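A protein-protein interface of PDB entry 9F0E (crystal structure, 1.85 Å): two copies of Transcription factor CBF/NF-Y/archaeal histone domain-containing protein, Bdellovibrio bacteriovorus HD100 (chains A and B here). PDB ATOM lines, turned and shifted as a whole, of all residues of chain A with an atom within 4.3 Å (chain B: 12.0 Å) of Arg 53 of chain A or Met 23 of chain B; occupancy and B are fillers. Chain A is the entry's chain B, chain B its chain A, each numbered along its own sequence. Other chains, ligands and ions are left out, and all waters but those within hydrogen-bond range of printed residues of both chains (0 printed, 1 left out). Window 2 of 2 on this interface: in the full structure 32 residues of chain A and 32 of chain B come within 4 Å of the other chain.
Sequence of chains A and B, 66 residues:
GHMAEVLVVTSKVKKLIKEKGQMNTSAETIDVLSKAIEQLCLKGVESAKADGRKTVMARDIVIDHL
Printed residues of chain A that touch a printed residue of chain B: Val 45, Ala 48, Lys 49, Arg 53, Lys 54, Thr 55 and Met 57. Along chain A the printed residues that touch a printed residue of chain B span positions 45 to 57. Hydrophobic or aromatic side chains of chain B within 4 Å of the printed part of chain A: Met 23. Among the printed residues, 10 pairs touch across the chains. Among the printed residues, no Asp or Glu carboxylate lies within 4 Å of a Lys or Arg side-chain nitrogen of the other chain.
The backbone carbonyl oxygen of Lys 54 of chain A is in hydrogen-bond range of the backbone NH of Asn 24 of chain B (2.9 Å). The side-chain hydroxyl (OG1) of Thr 29 of chain B lies close to the backbone carbonyl oxygen (O) of Met 57 of chain A (3.2 Å).
The side-chain hydroxyl (OG) of Ser 26 of chain B lies within hydrogen-bond range of the side-chain hydroxyl (OG1) of Thr 29 of chain B (2.8 Å). The backbone NH (N) of Arg 53 of chain A is in hydrogen-bond range of the backbone carbonyl oxygen (O) of Ala 48 of chain A (2.9 Å). The guanidinium group (NH1) of Arg 53 of chain A lies within hydrogen-bond range of the backbone carbonyl oxygen (O) of Thr 55 of chain A, at 3.0 Å. The guanidinium group of Arg 53 of chain A lies within hydrogen-bond range of the side-chain sulfur of Met 57 of chain A (3.6 Å). The guanidinium group (NH1) of Arg 53 of chain A is in salt-bridge range of the side-chain carboxylate (OD2) of Asp 60 of chain A, at 2.7 Å. The backbone NH (N) of Met 57 of chain A is in hydrogen-bond range of the side-chain carboxylate (OD2) of Asp 60 of chain A (2.9 Å).
Of the printed residues of chain B, Arg 53 of chain A touches Met 23 (2.8 Å). Of the printed residues of chain A, Met 23 of chain B touches Ala 48, Lys 49, Arg 53 and Lys 54. No residue of chain B comes within 4 Å of Ser 47 of chain A. Asp 51 of chain A touches none of the printed residues of chain B. Of chain B, only Asn 24 and Ser 26 come within 4 Å of Thr 55 of chain A. Printed residues of chain B within 4 Å of Met 57 of chain A: Ser 26 and Thr 29. No residue of chain B comes within 4 Å of Asp 60 of chain A. Of the printed residues of chain B, Val 45 of chain A touches Gly 21 (3.7 Å). Of the printed residues of chain A, Thr 29 of chain B touches Met 57 (2.8 Å). Printed residues of chain A within 4 Å of Ser 26 of chain B: Thr 55 (3.9 Å) and Met 57 (3.6 Å). Leu 16 of chain B touches none of the printed residues of chain A. Thr 10 of chain B touches none of the printed residues of chain A. The nearest printed residue of chain A that does not touch Met 23 of chain B is Val 45 of chain A (4.1 Å).
Gly 21 of chain B touches Val 45 of chain A (CA to CG1, 3.7 Å). Met 23 of chain B touches Ala 48 of chain A (CE to CB, 3.3 Å). Met 23 of chain B touches Lys 49 of chain A (CE to CG, 3.3 Å). CE of Met 23 of chain B touches O of Arg 53 of chain A (2.8 Å). Lys 54 of chain A touches Met 23 of chain B. Thr 55 of chain A touches Asn 24 of chain B. Ser 26 of chain B touches Thr 55 of chain A (N to CG2, 3.9 Å). Met 57 of chain A touches Ser 26 of chain B.
No position is printed for both chains. Of the 10 pairs that touch across the chains among the printed residues, none has its exchanged pair printed and touching as well.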
ATOM      1  N   VAL A  45     -24.347   0.708 -27.596  1.00  0.00           N
ATOM      2  CA  VAL A  45     -23.120   0.805 -26.760  1.00  0.00           C
ATOM      3  C   VAL A  45     -22.188   1.891 -27.329  1.00  0.00           C
ATOM      4  O   VAL A  45     -21.766   2.771 -26.534  1.00  0.00           O
ATOM      5  CB  VAL A  45     -22.434  -0.563 -26.608  1.00  0.00           C
ATOM      6  CG1 VAL A  45     -21.066  -0.435 -25.954  1.00  0.00           C
ATOM      7  CG2 VAL A  45     -23.314  -1.505 -25.797  1.00  0.00           C
ATOM      8  N   SER A  47     -22.714   4.524 -29.161  1.00  0.00           N
ATOM      9  CA  SER A  47     -23.367   5.853 -29.075  1.00  0.00           C
ATOM     10  C   SER A  47     -23.356   6.363 -27.630  1.00  0.00           C
ATOM     11  O   SER A  47     -22.933   7.530 -27.408  1.00  0.00           O
ATOM     12  CB  SER A  47     -24.784   5.783 -29.639  1.00  0.00           C
ATOM     13  OG  SER A  47     -25.460   6.992 -29.341  1.00  0.00           O
ATOM     14  N   ALA A  48     -23.726   5.517 -26.660  1.00  0.00           N
ATOM     15  CA  ALA A  48     -23.749   5.877 -25.220  1.00  0.00           C
ATOM     16  C   ALA A  48     -22.321   6.167 -24.726  1.00  0.00           C
ATOM     17  O   ALA A  48     -22.131   7.137 -23.950  1.00  0.00           O
ATOM     18  CB  ALA A  48     -24.375   4.764 -24.425  1.00  0.00           C
ATOM     19  N   LYS A  49     -21.337   5.377 -25.161  1.00  0.00           N
ATOM     20  CA  LYS A  49     -19.922   5.554 -24.729  1.00  0.00           C
ATOM     21  C   LYS A  49     -19.365   6.848 -25.306  1.00  0.00           C
ATOM     22  O   LYS A  49     -18.646   7.528 -24.592  1.00  0.00           O
ATOM     23  CB  LYS A  49     -19.050   4.380 -25.166  1.00  0.00           C
ATOM     24  CG  LYS A  49     -19.355   3.130 -24.364  1.00  0.00           C
ATOM     25  CD  LYS A  49     -18.236   2.200 -24.249  1.00  0.00           C
ATOM     26  CE  LYS A  49     -17.077   2.786 -23.492  1.00  0.00           C
ATOM     27  NZ  LYS A  49     -16.072   1.736 -23.277  1.00  0.00           N
ATOM     28  N   ASP A  51     -20.882   9.488 -25.825  1.00  0.00           N
ATOM     29  CA  ASP A  51     -21.528  10.586 -25.046  1.00  0.00           C
ATOM     30  C   ASP A  51     -21.104  10.513 -23.565  1.00  0.00           C
ATOM     31  O   ASP A  51     -21.630  11.313 -22.758  1.00  0.00           O
ATOM     32  CB  ASP A  51     -23.054  10.529 -25.197  1.00  0.00           C
ATOM     33  CG  ASP A  51     -23.788  11.860 -24.961  1.00  0.00           C
ATOM     34  OD1 ASP A  51     -23.323  12.893 -25.482  1.00  0.00           O
ATOM     35  OD2 ASP A  51     -24.856  11.854 -24.280  1.00  0.00           O
ATOM     36  N   GLY A  52     -20.226   9.578 -23.206  1.00  0.00           N
ATOM     37  CA  GLY A  52     -19.702   9.385 -21.837  1.00  0.00           C
ATOM     38  C   GLY A  52     -20.768   8.936 -20.842  1.00  0.00           C
ATOM     39  O   GLY A  52     -20.628   9.288 -19.642  1.00  0.00           O
ATOM     40  N   ARG A  53     -21.775   8.161 -21.277  1.00  0.00           N
ATOM     41  CA  ARG A  53     -22.838   7.656 -20.364  1.00  0.00           C
ATOM     42  C   ARG A  53     -22.581   6.199 -19.972  1.00  0.00           C
ATOM     43  O   ARG A  53     -21.872   5.514 -20.684  1.00  0.00           O
ATOM     44  CB  ARG A  53     -24.228   7.869 -20.971  1.00  0.00           C
ATOM     45  CG  ARG A  53     -24.704   9.316 -20.888  1.00  0.00           C
ATOM     46  CD  ARG A  53     -26.034   9.491 -21.594  1.00  0.00           C
ATOM     47  NE  ARG A  53     -25.914   9.525 -23.055  1.00  0.00           N
ATOM     48  CZ  ARG A  53     -26.320   8.573 -23.896  1.00  0.00           C
ATOM     49  NH1 ARG A  53     -26.839   7.439 -23.463  1.00  0.00           N
ATOM     50  NH2 ARG A  53     -26.179   8.758 -25.192  1.00  0.00           N
ATOM     51  N   LYS A  54     -23.174   5.761 -18.863  1.00  0.00           N
ATOM     52  CA  LYS A  54     -23.125   4.361 -18.368  1.00  0.00           C
ATOM     53  C   LYS A  54     -24.430   3.633 -18.695  1.00  0.00           C
ATOM     54  O   LYS A  54     -24.584   2.507 -18.207  1.00  0.00           O
ATOM     55  CB  LYS A  54     -22.949   4.326 -16.843  1.00  0.00           C
ATOM     56  N   THR A  55     -25.345   4.261 -19.444  1.00  0.00           N
ATOM     57  CA  THR A  55     -26.670   3.675 -19.783  1.00  0.00           C
ATOM     58  C   THR A  55     -26.929   3.833 -21.280  1.00  0.00           C
ATOM     59  O   THR A  55     -26.807   4.979 -21.791  1.00  0.00           O
ATOM     60  CB  THR A  55     -27.785   4.297 -18.937  1.00  0.00           C
ATOM     61  OG1 THR A  55     -27.457   4.137 -17.562  1.00  0.00           O
ATOM     62  CG2 THR A  55     -29.135   3.659 -19.186  1.00  0.00           C
ATOM     63  N   MET A  57     -29.620   4.261 -23.931  1.00  0.00           N
ATOM     64  CA  MET A  57     -30.966   4.894 -23.858  1.00  0.00           C
ATOM     65  C   MET A  57     -31.683   4.679 -25.197  1.00  0.00           C
ATOM     66  O   MET A  57     -31.019   4.261 -26.154  1.00  0.00           O
ATOM     67  CB  MET A  57     -30.829   6.380 -23.559  1.00  0.00           C
ATOM     68  CG  MET A  57     -30.102   6.607 -22.265  1.00  0.00           C
ATOM     69  SD  MET A  57     -29.892   8.338 -21.881  1.00  0.00           S
ATOM     70  CE  MET A  57     -31.607   8.797 -21.612  1.00  0.00           C
ATOM     71  N   ARG A  59     -32.511   6.853 -27.292  1.00  0.00           N
ATOM     72  CA  ARG A  59     -31.960   7.717 -28.371  1.00  0.00           C
ATOM     73  C   ARG A  59     -30.665   7.108 -28.950  1.00  0.00           C
ATOM     74  O   ARG A  59     -30.205   7.640 -29.980  1.00  0.00           O
ATOM     75  CB  ARG A  59     -31.744   9.158 -27.931  1.00  0.00           C
ATOM     76  CG  ARG A  59     -30.697   9.391 -26.847  1.00  0.00           C
ATOM     77  CD  ARG A  59     -30.363  10.862 -26.864  1.00  0.00           C
ATOM     78  NE  ARG A  59     -29.281  11.204 -25.967  1.00  0.00           N
ATOM     79  CZ  ARG A  59     -29.380  11.389 -24.654  1.00  0.00           C
ATOM     80  NH1 ARG A  59     -30.535  11.269 -24.024  1.00  0.00           N
ATOM     81  NH2 ARG A  59     -28.288  11.668 -23.971  1.00  0.00           N
ATOM     82  N   ASP A  60     -30.086   6.093 -28.302  1.00  0.00           N
ATOM     83  CA  ASP A  60     -28.858   5.390 -28.773  1.00  0.00           C
ATOM     84  C   ASP A  60     -29.186   4.301 -29.800  1.00  0.00           C
ATOM     85  O   ASP A  60     -28.228   3.800 -30.428  1.00  0.00           O
ATOM     86  CB  ASP A  60     -28.082   4.790 -27.603  1.00  0.00           C
ATOM     87  CG  ASP A  60     -27.538   5.879 -26.655  1.00  0.00           C
ATOM     88  OD1 ASP A  60     -27.040   6.905 -27.157  1.00  0.00           O
ATOM     89  OD2 ASP A  60     -27.660   5.715 -25.437  1.00  0.00           O
ATOM     90  N   THR B  10     -35.337  -9.566 -22.646  1.00  0.00           N
ATOM     91  CA  THR B  10     -34.761  -8.418 -21.893  1.00  0.00           C
ATOM     92  C   THR B  10     -33.478  -8.843 -21.163  1.00  0.00           C
ATOM     93  O   THR B  10     -32.499  -8.092 -21.238  1.00  0.00           O
ATOM     94  CB  THR B  10     -35.815  -7.832 -20.945  1.00  0.00           C
ATOM     95  OG1 THR B  10     -36.900  -7.397 -21.767  1.00  0.00           O
ATOM     96  CG2 THR B  10     -35.292  -6.692 -20.104  1.00  0.00           C
ATOM     97  N   SER B  11     -33.493  -9.962 -20.441  1.00  0.00           N
ATOM     98  CA  SER B  11     -32.360 -10.424 -19.592  1.00  0.00           C
ATOM     99  C   SER B  11     -31.114 -10.614 -20.463  1.00  0.00           C
ATOM    100  O   SER B  11     -30.010 -10.222 -20.025  1.00  0.00           O
ATOM    101  CB  SER B  11     -32.700 -11.686 -18.845  1.00  0.00           C
ATOM    102  OG  SER B  11     -32.961 -12.744 -19.750  1.00  0.00           O
ATOM    103  N   LYS B  12     -31.288 -11.181 -21.657  1.00  0.00           N
ATOM    104  CA  LYS B  12     -30.174 -11.467 -22.598  1.00  0.00           C
ATOM    105  C   LYS B  12     -29.690 -10.168 -23.251  1.00  0.00           C
ATOM    106  O   LYS B  12     -28.475 -10.057 -23.454  1.00  0.00           O
ATOM    107  CB  LYS B  12     -30.612 -12.485 -23.652  1.00  0.00           C
ATOM    108  CG  LYS B  12     -30.944 -13.867 -23.112  1.00  0.00           C
ATOM    109  CD  LYS B  12     -31.139 -14.882 -24.233  1.00  0.00           C
ATOM    110  CE  LYS B  12     -31.762 -16.184 -23.780  1.00  0.00           C
ATOM    111  NZ  LYS B  12     -30.960 -16.813 -22.710  1.00  0.00           N
ATOM    112  N   VAL B  13     -30.587  -9.225 -23.577  1.00  0.00           N
ATOM    113  CA  VAL B  13     -30.171  -7.915 -24.168  1.00  0.00           C
ATOM    114  C   VAL B  13     -29.334  -7.169 -23.113  1.00  0.00           C
ATOM    115  O   VAL B  13     -28.269  -6.603 -23.470  1.00  0.00           O
ATOM    116  CB  VAL B  13     -31.373  -7.070 -24.642  1.00  0.00           C
ATOM    117  CG1 VAL B  13     -31.000  -5.605 -24.813  1.00  0.00           C
ATOM    118  CG2 VAL B  13     -31.995  -7.612 -25.927  1.00  0.00           C
ATOM    119  N   LYS B  14     -29.791  -7.167 -21.859  1.00  0.00           N
ATOM    120  CA  LYS B  14     -29.095  -6.469 -20.743  1.00  0.00           C
ATOM    121  C   LYS B  14     -27.727  -7.127 -20.493  1.00  0.00           C
ATOM    122  O   LYS B  14     -26.767  -6.377 -20.312  1.00  0.00           O
ATOM    123  CB  LYS B  14     -29.961  -6.474 -19.482  1.00  0.00           C
ATOM    124  CG  LYS B  14     -31.210  -5.620 -19.586  1.00  0.00           C
ATOM    125  CD  LYS B  14     -31.957  -5.459 -18.284  1.00  0.00           C
ATOM    126  CE  LYS B  14     -32.850  -4.245 -18.291  1.00  0.00           C
ATOM    127  NZ  LYS B  14     -33.716  -4.224 -17.092  1.00  0.00           N
ATOM    128  N   LYS B  15     -27.657  -8.468 -20.494  1.00  0.00           N
ATOM    129  CA  LYS B  15     -26.404  -9.247 -20.280  1.00  0.00           C
ATOM    130  C   LYS B  15     -25.404  -8.887 -21.395  1.00  0.00           C
ATOM    131  O   LYS B  15     -24.240  -8.620 -21.063  1.00  0.00           O
ATOM    132  CB  LYS B  15     -26.713 -10.745 -20.215  1.00  0.00           C
ATOM    133  CG  LYS B  15     -25.516 -11.664 -19.980  1.00  0.00           C
ATOM    134  CD  LYS B  15     -25.742 -13.093 -20.455  1.00  0.00           C
ATOM    135  N   LEU B  16     -25.861  -8.803 -22.650  1.00  0.00           N
ATOM    136  CA  LEU B  16     -25.029  -8.436 -23.832  1.00  0.00           C
ATOM    137  C   LEU B  16     -24.460  -7.015 -23.680  1.00  0.00           C
ATOM    138  O   LEU B  16     -23.232  -6.825 -23.889  1.00  0.00           O
ATOM    139  CB  LEU B  16     -25.864  -8.527 -25.111  1.00  0.00           C
ATOM    140  CG  LEU B  16     -25.173  -7.962 -26.345  1.00  0.00           C
ATOM    141  CD1 LEU B  16     -23.933  -8.781 -26.677  1.00  0.00           C
ATOM    142  CD2 LEU B  16     -26.131  -7.915 -27.520  1.00  0.00           C
ATOM    143  N   ILE B  17     -25.306  -6.061 -23.311  1.00  0.00           N
ATOM    144  CA  ILE B  17     -24.915  -4.626 -23.191  1.00  0.00           C
ATOM    145  C   ILE B  17     -23.944  -4.452 -22.010  1.00  0.00           C
ATOM    146  O   ILE B  17     -22.978  -3.686 -22.163  1.00  0.00           O
ATOM    147  CB  ILE B  17     -26.158  -3.718 -23.105  1.00  0.00           C
ATOM    148  CG1 ILE B  17     -26.723  -3.477 -24.506  1.00  0.00           C
ATOM    149  CG2 ILE B  17     -25.833  -2.418 -22.381  1.00  0.00           C
ATOM    150  CD1 ILE B  17     -28.120  -2.882 -24.565  1.00  0.00           C
ATOM    151  N   LYS B  18     -24.190  -5.134 -20.890  1.00  0.00           N
ATOM    152  CA  LYS B  18     -23.335  -5.098 -19.670  1.00  0.00           C
ATOM    153  C   LYS B  18     -21.963  -5.709 -20.017  1.00  0.00           C
ATOM    154  O   LYS B  18     -20.922  -5.074 -19.724  1.00  0.00           O
ATOM    155  CB  LYS B  18     -24.004  -5.864 -18.520  1.00  0.00           C
ATOM    156  CG  LYS B  18     -23.275  -5.812 -17.181  1.00  0.00           C
ATOM    157  N   GLU B  19     -21.957  -6.881 -20.652  1.00  0.00           N
ATOM    158  CA  GLU B  19     -20.706  -7.640 -20.950  1.00  0.00           C
ATOM    159  C   GLU B  19     -19.853  -6.882 -21.973  1.00  0.00           C
ATOM    160  O   GLU B  19     -18.641  -6.812 -21.762  1.00  0.00           O
ATOM    161  CB  GLU B  19     -21.038  -9.048 -21.432  1.00  0.00           C
ATOM    162  CG  GLU B  19     -21.446  -9.961 -20.294  1.00  0.00           C
ATOM    163  CD  GLU B  19     -21.647 -11.418 -20.667  1.00  0.00           C
ATOM    164  OE1 GLU B  19     -21.823 -11.711 -21.871  1.00  0.00           O
ATOM    165  OE2 GLU B  19     -21.615 -12.259 -19.741  1.00  0.00           O
ATOM    166  N   LYS B  20     -20.467  -6.283 -22.993  1.00  0.00           N
ATOM    167  CA  LYS B  20     -19.764  -5.659 -24.145  1.00  0.00           C
ATOM    168  C   LYS B  20     -19.378  -4.203 -23.840  1.00  0.00           C
ATOM    169  O   LYS B  20     -18.306  -3.782 -24.338  1.00  0.00           O
ATOM    170  CB  LYS B  20     -20.633  -5.758 -25.407  1.00  0.00           C
ATOM    171  CG  LYS B  20     -20.829  -7.171 -25.929  1.00  0.00           C
ATOM    172  CD  LYS B  20     -19.585  -7.777 -26.506  1.00  0.00           C
ATOM    173  CE  LYS B  20     -19.786  -9.228 -26.883  1.00  0.00           C
ATOM    174  NZ  LYS B  20     -18.532  -9.838 -27.371  1.00  0.00           N
ATOM    175  N   GLY B  21     -20.183  -3.459 -23.067  1.00  0.00           N
ATOM    176  CA  GLY B  21     -19.949  -2.021 -22.817  1.00  0.00           C
ATOM    177  C   GLY B  21     -19.874  -1.647 -21.341  1.00  0.00           C
ATOM    178  O   GLY B  21     -19.752  -0.455 -21.069  1.00  0.00           O
ATOM    179  N   GLN B  22     -19.966  -2.611 -20.419  1.00  0.00           N
ATOM    180  CA  GLN B  22     -20.095  -2.377 -18.956  1.00  0.00           C
ATOM    181  C   GLN B  22     -21.192  -1.341 -18.691  1.00  0.00           C
ATOM    182  O   GLN B  22     -20.979  -0.455 -17.835  1.00  0.00           O
ATOM    183  CB  GLN B  22     -18.763  -1.899 -18.371  1.00  0.00           C
ATOM    184  CG  GLN B  22     -17.615  -2.871 -18.616  1.00  0.00           C
ATOM    185  CD  GLN B  22     -17.123  -2.864 -20.044  1.00  0.00           C
ATOM    186  OE1 GLN B  22     -16.826  -1.820 -20.623  1.00  0.00           O
ATOM    187  NE2 GLN B  22     -17.014  -4.049 -20.623  1.00  0.00           N
ATOM    188  N   MET B  23     -22.332  -1.412 -19.374  1.00  0.00           N
ATOM    189  CA  MET B  23     -23.394  -0.378 -19.226  1.00  0.00           C
ATOM    190  C   MET B  23     -24.732  -1.017 -18.876  1.00  0.00           C
ATOM    191  O   MET B  23     -24.910  -2.189 -19.194  1.00  0.00           O
ATOM    192  CB  MET B  23     -23.553   0.428 -20.512  1.00  0.00           C
ATOM    193  CG  MET B  23     -22.410   1.367 -20.746  1.00  0.00           C
ATOM    194  SD  MET B  23     -22.160   1.600 -22.496  1.00  0.00           S
ATOM    195  CE  MET B  23     -22.065   3.384 -22.532  1.00  0.00           C
ATOM    196  N   ASN B  24     -25.594  -0.232 -18.224  1.00  0.00           N
ATOM    197  CA  ASN B  24     -27.004  -0.570 -17.950  1.00  0.00           C
ATOM    198  C   ASN B  24     -27.803  -0.313 -19.236  1.00  0.00           C
ATOM    199  O   ASN B  24     -27.272   0.306 -20.193  1.00  0.00           O
ATOM    200  CB  ASN B  24     -27.574   0.202 -16.756  1.00  0.00           C
ATOM    201  CG  ASN B  24     -26.805  -0.036 -15.470  1.00  0.00           C
ATOM    202  OD1 ASN B  24     -26.041  -0.989 -15.356  1.00  0.00           O
ATOM    203  ND2 ASN B  24     -26.977   0.835 -14.496  1.00  0.00           N
ATOM    204  N   THR B  25     -29.053  -0.753 -19.233  1.00  0.00           N
ATOM    205  CA  THR B  25     -29.984  -0.626 -20.379  1.00  0.00           C
ATOM    206  C   THR B  25     -31.293  -0.034 -19.857  1.00  0.00           C
ATOM    207  O   THR B  25     -31.854  -0.623 -18.929  1.00  0.00           O
ATOM    208  CB  THR B  25     -30.202  -1.995 -21.034  1.00  0.00           C
ATOM    209  OG1 THR B  25     -28.940  -2.577 -21.358  1.00  0.00           O
ATOM    210  CG2 THR B  25     -31.049  -1.935 -22.286  1.00  0.00           C
ATOM    211  N   SER B  26     -31.746   1.090 -20.408  1.00  0.00           N
ATOM    212  CA  SER B  26     -33.001   1.744 -19.953  1.00  0.00           C
ATOM    213  C   SER B  26     -34.213   0.897 -20.366  1.00  0.00           C
ATOM    214  O   SER B  26     -34.126   0.076 -21.327  1.00  0.00           O
ATOM    215  CB  SER B  26     -33.086   3.176 -20.415  1.00  0.00           C
ATOM    216  OG  SER B  26     -33.436   3.264 -21.777  1.00  0.00           O
ATOM    217  N   ALA B  27     -35.313   1.040 -19.626  1.00  0.00           N
ATOM    218  CA  ALA B  27     -36.607   0.400 -19.946  1.00  0.00           C
ATOM    219  C   ALA B  27     -36.995   0.801 -21.373  1.00  0.00           C
ATOM    220  O   ALA B  27     -37.457  -0.085 -22.137  1.00  0.00           O
ATOM    221  CB  ALA B  27     -37.655   0.815 -18.924  1.00  0.00           C
ATOM    222  N   GLU B  28     -36.804   2.080 -21.718  1.00  0.00           N
ATOM    223  CA  GLU B  28     -37.198   2.666 -23.026  1.00  0.00           C
ATOM    224  C   GLU B  28     -36.347   2.063 -24.154  1.00  0.00           C
ATOM    225  O   GLU B  28     -36.863   1.923 -25.276  1.00  0.00           O
ATOM    226  CB  GLU B  28     -37.098   4.189 -23.003  1.00  0.00           C
ATOM    227  CG  GLU B  28     -38.140   4.841 -22.105  1.00  0.00           C
ATOM    228  CD  GLU B  28     -37.750   5.005 -20.640  1.00  0.00           C
ATOM    229  OE1 GLU B  28     -36.663   4.561 -20.231  1.00  0.00           O
ATOM    230  OE2 GLU B  28     -38.555   5.557 -19.910  1.00  0.00           O
ATOM    231  N   THR B  29     -35.095   1.677 -23.880  1.00  0.00           N
ATOM    232  CA  THR B  29     -34.255   0.972 -24.898  1.00  0.00           C
ATOM    233  C   THR B  29     -34.901  -0.373 -25.287  1.00  0.00           C
ATOM    234  O   THR B  29     -34.965  -0.697 -26.495  1.00  0.00           O
ATOM    235  CB  THR B  29     -32.809   0.850 -24.412  1.00  0.00           C
ATOM    236  OG1 THR B  29     -32.305   2.156 -24.126  1.00  0.00           O
ATOM    237  CG2 THR B  29     -31.884   0.193 -25.406  1.00  0.00           C
ATOM    238  N   ILE B  30     -35.341  -1.157 -24.305  1.00  0.00           N
ATOM    239  CA  ILE B  30     -36.055  -2.453 -24.526  1.00  0.00           C
ATOM    240  C   ILE B  30     -37.290  -2.194 -25.398  1.00  0.00           C
ATOM    241  O   ILE B  30     -37.534  -2.973 -26.376  1.00  0.00           O
ATOM    242  CB  ILE B  30     -36.409  -3.093 -23.168  1.00  0.00           C
ATOM    243  CG1 ILE B  30     -35.166  -3.356 -22.310  1.00  0.00           C
ATOM    244  CG2 ILE B  30     -37.266  -4.340 -23.331  1.00  0.00           C
ATOM    245  CD1 ILE B  30     -34.115  -4.241 -22.925  1.00  0.00           C
ATOM    246  N   VAL B  32     -37.813   0.252 -27.574  1.00  0.00           N
ATOM    247  CA  VAL B  32     -37.416   0.602 -28.971  1.00  0.00           C
ATOM    248  C   VAL B  32     -37.027  -0.696 -29.705  1.00  0.00           C
ATOM    249  O   VAL B  32     -37.423  -0.845 -30.878  1.00  0.00           O
ATOM    250  CB  VAL B  32     -36.296   1.663 -29.031  1.00  0.00           C
ATOM    251  CG1 VAL B  32     -35.923   1.975 -30.482  1.00  0.00           C
ATOM    252  CG2 VAL B  32     -36.687   2.950 -28.328  1.00  0.00           C
ATOM    253  N   LEU B  33     -36.324  -1.620 -29.025  1.00  0.00           N
ATOM    254  CA  LEU B  33     -35.875  -2.906 -29.628  1.00  0.00           C
ATOM    255  C   LEU B  33     -37.105  -3.757 -29.976  1.00  0.00           C
ATOM    256  O   LEU B  33     -37.108  -4.326 -31.080  1.00  0.00           O
ATOM    257  CB  LEU B  33     -34.914  -3.629 -28.685  1.00  0.00           C
ATOM    258  CG  LEU B  33     -33.562  -2.931 -28.510  1.00  0.00           C
ATOM    259  CD1 LEU B  33     -32.733  -3.600 -27.436  1.00  0.00           C
ATOM    260  CD2 LEU B  33     -32.794  -2.899 -29.830  1.00  0.00           C
